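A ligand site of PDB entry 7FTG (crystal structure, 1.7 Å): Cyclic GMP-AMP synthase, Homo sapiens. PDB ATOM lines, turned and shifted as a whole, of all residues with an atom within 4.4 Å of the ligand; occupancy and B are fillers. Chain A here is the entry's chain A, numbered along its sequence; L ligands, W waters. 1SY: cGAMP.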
ATOM      1  N   ASP A  67      -3.129   3.151  12.891  1.00  0.00           N
ATOM      2  CA  ASP A  67      -2.768   2.584  11.597  1.00  0.00           C
ATOM      3  C   ASP A  67      -1.627   3.388  10.999  1.00  0.00           C
ATOM      4  O   ASP A  67      -1.760   4.601  10.798  1.00  0.00           O
ATOM      5  CB  ASP A  67      -3.975   2.568  10.655  1.00  0.00           C
ATOM      6  CG  ASP A  67      -3.608   2.237   9.222  1.00  0.00           C
ATOM      7  OD1 ASP A  67      -3.177   3.151   8.480  1.00  0.00           O
ATOM      8  OD2 ASP A  67      -3.732   1.054   8.852  1.00  0.00           O
ATOM      9  N   TYR A  88      -5.872  -8.188  -6.372  1.00  0.00           N
ATOM     10  CA  TYR A  88      -4.673  -8.913  -5.963  1.00  0.00           C
ATOM     11  C   TYR A  88      -3.783  -9.190  -7.168  1.00  0.00           C
ATOM     12  O   TYR A  88      -4.276  -9.498  -8.265  1.00  0.00           O
ATOM     13  CB  TYR A  88      -5.051 -10.232  -5.281  1.00  0.00           C
ATOM     14  CG  TYR A  88      -5.864 -10.043  -4.027  1.00  0.00           C
ATOM     15  CD1 TYR A  88      -7.240  -9.946  -4.078  1.00  0.00           C
ATOM     16  CD2 TYR A  88      -5.236  -9.942  -2.774  1.00  0.00           C
ATOM     17  CE1 TYR A  88      -7.997  -9.760  -2.936  1.00  0.00           C
ATOM     18  CE2 TYR A  88      -5.984  -9.760  -1.623  1.00  0.00           C
ATOM     19  CZ  TYR A  88      -7.355  -9.672  -1.715  1.00  0.00           C
ATOM     20  OH  TYR A  88      -8.122  -9.481  -0.583  1.00  0.00           O
ATOM     21  N   ARG A 142      -5.788 -10.576  13.552  1.00  0.00           N
ATOM     22  CA  ARG A 142      -6.476 -11.611  12.784  1.00  0.00           C
ATOM     23  C   ARG A 142      -5.559 -12.235  11.745  1.00  0.00           C
ATOM     24  O   ARG A 142      -4.359 -11.963  11.697  1.00  0.00           O
ATOM     25  CB  ARG A 142      -7.714 -11.042  12.100  1.00  0.00           C
ATOM     26  CG  ARG A 142      -8.855 -10.697  13.030  1.00  0.00           C
ATOM     27  CD  ARG A 142      -9.992 -10.043  12.260  1.00  0.00           C
ATOM     28  NE  ARG A 142     -11.073  -9.587  13.127  1.00  0.00           N
ATOM     29  CZ  ARG A 142     -12.070  -8.813  12.726  1.00  0.00           C
ATOM     30  NH1 ARG A 142     -12.126  -8.387  11.472  1.00  0.00           N
ATOM     31  NH2 ARG A 142     -13.013  -8.444  13.590  1.00  0.00           N
ATOM     32  N   GLY A 143      -6.155 -13.073  10.893  1.00  0.00           N
ATOM     33  CA  GLY A 143      -5.445 -13.755   9.836  1.00  0.00           C
ATOM     34  C   GLY A 143      -5.684 -13.119   8.488  1.00  0.00           C
ATOM     35  O   GLY A 143      -6.740 -12.549   8.230  1.00  0.00           O
ATOM     36  N   GLY A 144      -4.684 -13.228   7.607  1.00  0.00           N
ATOM     37  CA  GLY A 144      -4.752 -12.631   6.299  1.00  0.00           C
ATOM     38  C   GLY A 144      -4.415 -11.153   6.248  1.00  0.00           C
ATOM     39  O   GLY A 144      -4.480 -10.564   5.171  1.00  0.00           O
ATOM     40  N   SER A 145      -4.057 -10.535   7.380  1.00  0.00           N
ATOM     41  CA  SER A 145      -3.783  -9.106   7.316  1.00  0.00           C
ATOM     42  C   SER A 145      -2.391  -8.825   6.749  1.00  0.00           C
ATOM     43  O   SER A 145      -1.458  -9.591   6.973  1.00  0.00           O
ATOM     44  CB  SER A 145      -3.895  -8.472   8.698  1.00  0.00           C
ATOM     45  OG  SER A 145      -3.489  -7.118   8.632  1.00  0.00           O
ATOM     46  N   PRO A 146      -2.247  -7.711   6.016  1.00  0.00           N
ATOM     47  CA  PRO A 146      -0.921  -7.244   5.610  1.00  0.00           C
ATOM     48  C   PRO A 146      -0.161  -6.557   6.723  1.00  0.00           C
ATOM     49  O   PRO A 146       1.015  -6.209   6.522  1.00  0.00           O
ATOM     50  CB  PRO A 146      -1.240  -6.249   4.491  1.00  0.00           C
ATOM     51  CG  PRO A 146      -2.539  -5.643   4.968  1.00  0.00           C
ATOM     52  CD  PRO A 146      -3.309  -6.770   5.602  1.00  0.00           C
ATOM     53  N   ALA A 147      -0.815  -6.325   7.855  1.00  0.00           N
ATOM     54  CA  ALA A 147      -0.272  -5.529   8.947  1.00  0.00           C
ATOM     55  C   ALA A 147       0.459  -6.387   9.964  1.00  0.00           C
ATOM     56  O   ALA A 147       0.176  -7.583  10.131  1.00  0.00           O
ATOM     57  CB  ALA A 147      -1.387  -4.744   9.647  1.00  0.00           C
ATOM     58  N   ASP A 159      -1.522  -1.039  13.978  1.00  0.00           N
ATOM     59  CA  ASP A 159      -1.158  -1.812  12.805  1.00  0.00           C
ATOM     60  C   ASP A 159      -0.030  -1.098  12.058  1.00  0.00           C
ATOM     61  O   ASP A 159      -0.133   0.100  11.764  1.00  0.00           O
ATOM     62  CB  ASP A 159      -2.350  -1.985  11.867  1.00  0.00           C
ATOM     63  CG  ASP A 159      -3.398  -2.950  12.396  1.00  0.00           C
ATOM     64  OD1 ASP A 159      -3.319  -3.357  13.570  1.00  0.00           O
ATOM     65  OD2 ASP A 159      -4.305  -3.303  11.611  1.00  0.00           O
ATOM     66  N   THR A 161       1.920  -1.483   8.471  1.00  0.00           N
ATOM     67  CA  THR A 161       1.743  -2.161   7.186  1.00  0.00           C
ATOM     68  C   THR A 161       2.852  -1.756   6.219  1.00  0.00           C
ATOM     69  O   THR A 161       3.048  -0.572   5.953  1.00  0.00           O
ATOM     70  CB  THR A 161       0.374  -1.861   6.601  1.00  0.00           C
ATOM     71  OG1 THR A 161      -0.633  -2.426   7.449  1.00  0.00           O
ATOM     72  CG2 THR A 161       0.248  -2.442   5.203  1.00  0.00           C
ATOM     73  N   VAL A 200       0.138  -3.827  -0.716  1.00  0.00           N
ATOM     74  CA  VAL A 200       0.391  -4.317   0.625  1.00  0.00           C
ATOM     75  C   VAL A 200       0.392  -5.844   0.559  1.00  0.00           C
ATOM     76  O   VAL A 200      -0.292  -6.408  -0.305  1.00  0.00           O
ATOM     77  CB  VAL A 200      -0.636  -3.775   1.630  1.00  0.00           C
ATOM     78  CG1 VAL A 200      -0.511  -2.252   1.671  1.00  0.00           C
ATOM     79  CG2 VAL A 200      -2.061  -4.146   1.204  1.00  0.00           C
ATOM     80  N   LYS A 202      -1.187  -8.255   1.562  1.00  0.00           N
ATOM     81  CA  LYS A 202      -2.412  -8.986   1.808  1.00  0.00           C
ATOM     82  C   LYS A 202      -2.577  -9.961   0.665  1.00  0.00           C
ATOM     83  O   LYS A 202      -2.492  -9.575  -0.507  1.00  0.00           O
ATOM     84  CB  LYS A 202      -3.615  -8.029   1.884  1.00  0.00           C
ATOM     85  CG  LYS A 202      -4.934  -8.662   1.510  1.00  0.00           C
ATOM     86  CD  LYS A 202      -5.526  -9.407   2.677  1.00  0.00           C
ATOM     87  CE  LYS A 202      -6.545 -10.446   2.252  1.00  0.00           C
ATOM     88  NZ  LYS A 202      -6.942 -11.320   3.390  1.00  0.00           N
ATOM     89  N   ARG A 216      -2.022  -6.748  -2.545  1.00  0.00           N
ATOM     90  CA  ARG A 216      -3.280  -6.085  -2.827  1.00  0.00           C
ATOM     91  C   ARG A 216      -3.033  -4.593  -3.005  1.00  0.00           C
ATOM     92  O   ARG A 216      -2.182  -4.003  -2.336  1.00  0.00           O
ATOM     93  CB  ARG A 216      -4.301  -6.320  -1.717  1.00  0.00           C
ATOM     94  CG  ARG A 216      -5.729  -6.188  -2.214  1.00  0.00           C
ATOM     95  CD  ARG A 216      -6.636  -5.690  -1.118  1.00  0.00           C
ATOM     96  NE  ARG A 216      -6.080  -4.494  -0.501  1.00  0.00           N
ATOM     97  CZ  ARG A 216      -5.950  -4.328   0.807  1.00  0.00           C
ATOM     98  NH1 ARG A 216      -6.395  -5.266   1.638  1.00  0.00           N
ATOM     99  NH2 ARG A 216      -5.428  -3.193   1.289  1.00  0.00           N
ATOM    100  N   LEU A 217      -3.746  -4.006  -3.958  1.00  0.00           N
ATOM    101  CA  LEU A 217      -3.661  -2.566  -4.165  1.00  0.00           C
ATOM    102  C   LEU A 217      -4.128  -1.825  -2.910  1.00  0.00           C
ATOM    103  O   LEU A 217      -5.038  -2.277  -2.196  1.00  0.00           O
ATOM    104  CB  LEU A 217      -4.515  -2.131  -5.348  1.00  0.00           C
ATOM    105  CG  LEU A 217      -4.111  -2.710  -6.705  1.00  0.00           C
ATOM    106  CD1 LEU A 217      -5.150  -2.363  -7.749  1.00  0.00           C
ATOM    107  CD2 LEU A 217      -2.757  -2.147  -7.093  1.00  0.00           C
ATOM    108  N   SER A 218      -3.510  -0.677  -2.662  1.00  0.00           N
ATOM    109  CA  SER A 218      -3.918   0.195  -1.578  1.00  0.00           C
ATOM    110  C   SER A 218      -3.799   1.633  -2.048  1.00  0.00           C
ATOM    111  O   SER A 218      -2.832   2.004  -2.711  1.00  0.00           O
ATOM    112  CB  SER A 218      -3.068  -0.018  -0.323  1.00  0.00           C
ATOM    113  OG  SER A 218      -3.356   0.990   0.639  1.00  0.00           O
ATOM    114  N   SER A 220      -4.603   4.271   0.346  1.00  0.00           N
ATOM    115  CA  SER A 220      -4.850   4.969   1.598  1.00  0.00           C
ATOM    116  C   SER A 220      -4.470   6.453   1.516  1.00  0.00           C
ATOM    117  O   SER A 220      -5.119   7.285   2.152  1.00  0.00           O
ATOM    118  CB  SER A 220      -4.083   4.290   2.742  1.00  0.00           C
ATOM    119  OG  SER A 220      -4.667   3.038   3.075  1.00  0.00           O
ATOM    120  N   SER A 274     -16.149  -3.433   9.471  1.00  0.00           N
ATOM    121  CA  SER A 274     -14.987  -2.597   9.710  1.00  0.00           C
ATOM    122  C   SER A 274     -15.302  -1.141   9.399  1.00  0.00           C
ATOM    123  O   SER A 274     -16.179  -0.835   8.586  1.00  0.00           O
ATOM    124  CB  SER A 274     -13.802  -3.062   8.848  1.00  0.00           C
ATOM    125  OG  SER A 274     -12.786  -2.080   8.794  1.00  0.00           O
ATOM    126  N   TYR A 276     -13.497   0.457   7.606  1.00  0.00           N
ATOM    127  CA  TYR A 276     -13.210   0.610   6.182  1.00  0.00           C
ATOM    128  C   TYR A 276     -14.466   0.423   5.326  1.00  0.00           C
ATOM    129  O   TYR A 276     -14.606   1.059   4.287  1.00  0.00           O
ATOM    130  CB  TYR A 276     -12.114  -0.382   5.725  1.00  0.00           C
ATOM    131  CG  TYR A 276     -11.624  -0.021   4.335  1.00  0.00           C
ATOM    132  CD1 TYR A 276     -10.756   1.053   4.144  1.00  0.00           C
ATOM    133  CD2 TYR A 276     -12.041  -0.734   3.206  1.00  0.00           C
ATOM    134  CE1 TYR A 276     -10.317   1.424   2.877  1.00  0.00           C
ATOM    135  CE2 TYR A 276     -11.606  -0.371   1.928  1.00  0.00           C
ATOM    136  CZ  TYR A 276     -10.742   0.711   1.779  1.00  0.00           C
ATOM    137  OH  TYR A 276     -10.304   1.083   0.511  1.00  0.00           O
ATOM    138  N   HIS A 277     -15.401  -0.429   5.771  1.00  0.00           N
ATOM    139  CA  HIS A 277     -16.669  -0.590   5.049  1.00  0.00           C
ATOM    140  C   HIS A 277     -17.491   0.681   5.110  1.00  0.00           C
ATOM    141  O   HIS A 277     -18.075   1.112   4.118  1.00  0.00           O
ATOM    142  CB  HIS A 277     -17.455  -1.751   5.650  1.00  0.00           C
ATOM    143  CG  HIS A 277     -16.775  -3.065   5.489  1.00  0.00           C
ATOM    144  ND1 HIS A 277     -16.642  -3.968   6.523  1.00  0.00           N
ATOM    145  CD2 HIS A 277     -16.193  -3.629   4.408  1.00  0.00           C
ATOM    146  CE1 HIS A 277     -15.993  -5.031   6.075  1.00  0.00           C
ATOM    147  NE2 HIS A 277     -15.718  -4.853   4.796  1.00  0.00           N
ATOM    148  N   ASN A 322     -15.379  -1.634  -3.664  1.00  0.00           N
ATOM    149  CA  ASN A 322     -14.173  -0.863  -3.373  1.00  0.00           C
ATOM    150  C   ASN A 322     -14.221   0.411  -4.214  1.00  0.00           C
ATOM    151  O   ASN A 322     -14.602   0.377  -5.389  1.00  0.00           O
ATOM    152  CB  ASN A 322     -12.937  -1.718  -3.671  1.00  0.00           C
ATOM    153  CG  ASN A 322     -11.611  -0.994  -3.399  1.00  0.00           C
ATOM    154  OD1 ASN A 322     -11.294  -0.028  -4.082  1.00  0.00           O
ATOM    155  ND2 ASN A 322     -10.838  -1.488  -2.420  1.00  0.00           N
ATOM    156  N   PHE A 328     -14.196  -5.203  -7.216  1.00  0.00           N
ATOM    157  CA  PHE A 328     -13.859  -5.869  -5.976  1.00  0.00           C
ATOM    158  C   PHE A 328     -14.985  -5.579  -4.982  1.00  0.00           C
ATOM    159  O   PHE A 328     -15.122  -4.450  -4.517  1.00  0.00           O
ATOM    160  CB  PHE A 328     -12.510  -5.412  -5.439  1.00  0.00           C
ATOM    161  CG  PHE A 328     -12.047  -6.191  -4.234  1.00  0.00           C
ATOM    162  CD1 PHE A 328     -11.562  -7.483  -4.376  1.00  0.00           C
ATOM    163  CD2 PHE A 328     -12.096  -5.648  -2.974  1.00  0.00           C
ATOM    164  CE1 PHE A 328     -11.142  -8.214  -3.275  1.00  0.00           C
ATOM    165  CE2 PHE A 328     -11.676  -6.380  -1.863  1.00  0.00           C
ATOM    166  CZ  PHE A 328     -11.197  -7.659  -2.014  1.00  0.00           C
ATOM    167  N   LEU A 330     -16.489  -5.740  -1.494  1.00  0.00           N
ATOM    168  CA  LEU A 330     -16.145  -5.926  -0.087  1.00  0.00           C
ATOM    169  C   LEU A 330     -17.199  -6.755   0.657  1.00  0.00           C
ATOM    170  O   LEU A 330     -16.894  -7.329   1.706  1.00  0.00           O
ATOM    171  CB  LEU A 330     -15.963  -4.577   0.619  1.00  0.00           C
ATOM    172  CG  LEU A 330     -14.939  -3.626  -0.021  1.00  0.00           C
ATOM    173  CD1 LEU A 330     -14.946  -2.251   0.614  1.00  0.00           C
ATOM    174  CD2 LEU A 330     -13.571  -4.240   0.051  1.00  0.00           C
ATOM    175  N   LEU A 335     -16.115 -13.023   1.453  1.00  0.00           N
ATOM    176  CA  LEU A 335     -15.485 -12.248   2.519  1.00  0.00           C
ATOM    177  C   LEU A 335     -16.336 -12.131   3.768  1.00  0.00           C
ATOM    178  O   LEU A 335     -15.805 -12.141   4.883  1.00  0.00           O
ATOM    179  CB  LEU A 335     -15.154 -10.839   2.019  1.00  0.00           C
ATOM    180  CG  LEU A 335     -14.146 -10.715   0.878  1.00  0.00           C
ATOM    181  CD1 LEU A 335     -14.038  -9.256   0.451  1.00  0.00           C
ATOM    182  CD2 LEU A 335     -12.792 -11.245   1.320  1.00  0.00           C
HETATM  183  C2  1SY L   1      -8.006  -1.335   0.848  1.00  0.00           C
HETATM  184  N01 1SY L   1      -6.277   0.297   3.645  1.00  0.00           N
HETATM  185  C6  1SY L   1      -7.197  -0.594   2.910  1.00  0.00           C
HETATM  186  N1  1SY L   1      -7.190  -0.543   1.578  1.00  0.00           N
HETATM  187  N3  1SY L   1      -8.835  -2.202   1.489  1.00  0.00           N
HETATM  188  C4  1SY L   1      -8.842  -2.254   2.822  1.00  0.00           C
HETATM  189  C5  1SY L   1      -8.035  -1.457   3.552  1.00  0.00           C
HETATM  190  N7  1SY L   1      -8.244  -1.719   4.871  1.00  0.00           N
HETATM  191  C8  1SY L   1      -9.211  -2.671   4.977  1.00  0.00           C
HETATM  192  N9  1SY L   1      -9.543  -2.976   3.713  1.00  0.00           N
HETATM  193  C1' 1SY L   1     -10.555  -3.943   3.296  1.00  0.00           C
HETATM  194  C2' 1SY L   1     -10.008  -5.323   3.133  1.00  0.00           C
HETATM  195  O2' 1SY L   1     -10.476  -5.811   1.867  1.00  0.00           O
HETATM  196  C3' 1SY L   1     -10.529  -6.107   4.303  1.00  0.00           C
HETATM  197  C4' 1SY L   1     -11.686  -5.402   4.735  1.00  0.00           C
HETATM  198  C16 1SY L   1     -11.855  -5.492   6.261  1.00  0.00           C
HETATM  199  O17 1SY L   1     -10.787  -4.780   6.893  1.00  0.00           O
HETATM  200  P18 1SY L   1     -10.470  -4.926   8.596  1.00  0.00           P
HETATM  201  O19 1SY L   1     -10.717  -3.691   9.347  1.00  0.00           O
HETATM  202  O20 1SY L   1      -8.896  -5.589   8.937  1.00  0.00           O
HETATM  203  C21 1SY L   1      -8.590  -6.565   7.897  1.00  0.00           C
HETATM  204  C22 1SY L   1      -8.872  -7.927   8.380  1.00  0.00           C
HETATM  205  O23 1SY L   1      -8.525  -8.014   9.736  1.00  0.00           O
HETATM  206  C24 1SY L   1      -7.927  -8.834   7.615  1.00  0.00           C
HETATM  207  C25 1SY L   1      -8.538  -9.401   6.427  1.00  0.00           C
HETATM  208  O26 1SY L   1      -9.571  -8.472   5.891  1.00  0.00           O
HETATM  209  P27 1SY L   1      -9.733  -8.649   4.211  1.00  0.00           P
HETATM  210  O28 1SY L   1     -10.940  -7.464   3.897  1.00  0.00           O
HETATM  211  O29 1SY L   1      -8.448  -8.209   3.542  1.00  0.00           O
HETATM  212  O30 1SY L   1     -10.002 -10.047   3.745  1.00  0.00           O
HETATM  213  O31 1SY L   1      -6.789  -7.970   7.234  1.00  0.00           O
HETATM  214  C32 1SY L   1      -7.195  -6.615   7.670  1.00  0.00           C
HETATM  215  N33 1SY L   1      -6.702  -5.661   6.678  1.00  0.00           N
HETATM  216  C34 1SY L   1      -7.002  -6.022   5.408  1.00  0.00           C
HETATM  217  N35 1SY L   1      -6.450  -5.065   4.615  1.00  0.00           N
HETATM  218  C36 1SY L   1      -5.992  -4.564   6.697  1.00  0.00           C
HETATM  219  C37 1SY L   1      -5.822  -4.160   5.413  1.00  0.00           C
HETATM  220  C38 1SY L   1      -5.031  -2.889   5.164  1.00  0.00           C
HETATM  221  N39 1SY L   1      -4.497  -2.180   6.308  1.00  0.00           N
HETATM  222  C40 1SY L   1      -4.693  -2.631   7.639  1.00  0.00           C
HETATM  223  N41 1SY L   1      -4.143  -1.886   8.796  1.00  0.00           N
HETATM  224  N42 1SY L   1      -5.445  -3.830   7.873  1.00  0.00           N
HETATM  225  O43 1SY L   1      -4.837  -2.454   4.042  1.00  0.00           O
HETATM  226  O44 1SY L   1     -11.414  -5.900   9.131  1.00  0.00           O
HETATM  227  O4' 1SY L   1     -11.551  -3.986   4.313  1.00  0.00           O
HETATM  228  O   HOH W   1      -7.998  -0.200  -2.270  1.00  0.00           O
HETATM  229  O   HOH W   2      -8.477  -7.387   1.139  1.00  0.00           O
HETATM  230  O   HOH W   3     -13.643  -8.903   4.924  1.00  0.00           O
HETATM  231  O   HOH W   4      -7.151   1.504  -0.419  1.00  0.00           O
HETATM  232  O   HOH W   5      -3.352  -0.359   3.002  1.00  0.00           O
HETATM  233  O   HOH W   6     -10.164  -3.502  -0.577  1.00  0.00           O
HETATM  234  O   HOH W   7      -3.050   0.223   6.043  1.00  0.00           O
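NH1 of Arg 142 is in salt-bridge range of O44 of the ligand, 3.5 Å away.
NZ of Lys 202 is in salt-bridge range of O30 of the ligand (3.3 Å).
The side-chain carboxylate of Asp 67 is in hydrogen-bond range of a nitrogen (N41) of the ligand (3.0 Å).
N01 of the ligand is in hydrogen-bond range of OG of Ser 220.
The guanidinium group (NH2) of Arg 216 is in hydrogen-bond range of an oxygen (O43) of the ligand, 2.9 Å away.
The side-chain hydroxyl of Ser 274 is in hydrogen-bond range of an oxygen (O19) of the ligand (2.7 Å).
N41 of the ligand is in hydrogen-bond range of OD2 of Asp 159, 3.2 Å away.
OG of Ser 220 is in hydrogen-bond range of OG of Ser 218, at 3.4 Å.
A ring nitrogen (ND1) of His 277 sits at hydrogen-bond distance from the backbone NH (N) of Ser 274 (3.0 Å).
The backbone NH (N) of Tyr 276 is in hydrogen-bond range of the side-chain hydroxyl (OG) of Ser 274 (2.9 Å).
The side-chain hydroxyl (OG) of Ser 145 is in hydrogen-bond range of the backbone NH (N) of Ala 147 (2.9 Å).
N of Asn 322 is in hydrogen-bond range of O of Phe 328 (3.0 Å).
The backbone carbonyl oxygen (O) of Arg 216 sits at hydrogen-bond distance from the backbone NH (N) of Val 200 (2.8 Å).
O of Gly 144 lies close to NZ of Lys 202 (3.1 Å).
Gly 143 touches the ligand (O to C24, 3.9 Å).
Ser 145 touches the ligand (CA to O31, 3.2 Å).
Pro 146 touches the ligand.
OG1 of Thr 161 touches N41 of the ligand, at 3.8 Å.
Tyr 276 touches the ligand.
CE2 of Phe 328 touches O2' of the ligand, 3.96 Å away.
CD2 of Leu 330 touches O2' of the ligand, 3.9 Å away.
Leu 335 touches the ligand.
Hydrophobic or aromatic side chains that line the ligand: Pro 146, Tyr 276, Phe 328, Leu 330 and Leu 335.
15 residues have an atom within 4 Å of the ligand: Asp 67, Arg 142, Gly 143, Ser 145, Pro 146, Asp 159, Thr 161, Lys 202, Arg 216, Ser 220, Ser 274, Tyr 276, Phe 328, Leu 330 and Leu 335.
The nearest printed residue that does not touch the ligand is Gly 144 (4.04 Å).
Water W2 lies within hydrogen-bond range of O29 of the ligand (2.5 Å), OH of Tyr 88 (2.7 Å) and NH1 of Arg 216 (3.0 Å).
Water W5 bridges OG of Ser 218 (2.7 Å) and O43 of the ligand (2.8 Å).
Water W6 bridges a nitrogen (N3) of the ligand (2.8 Å) and the side-chain amide nitrogen (ND2) of Asn 322 (2.8 Å).
Water W7 lies within hydrogen-bond range of N39 of the ligand (2.8 Å) and OD2 of Asp 67 (3.0 Å).
Water W4 bridges a nitrogen (N1) of the ligand (2.9 Å) and the side-chain hydroxyl of Tyr 276 (3.3 Å).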
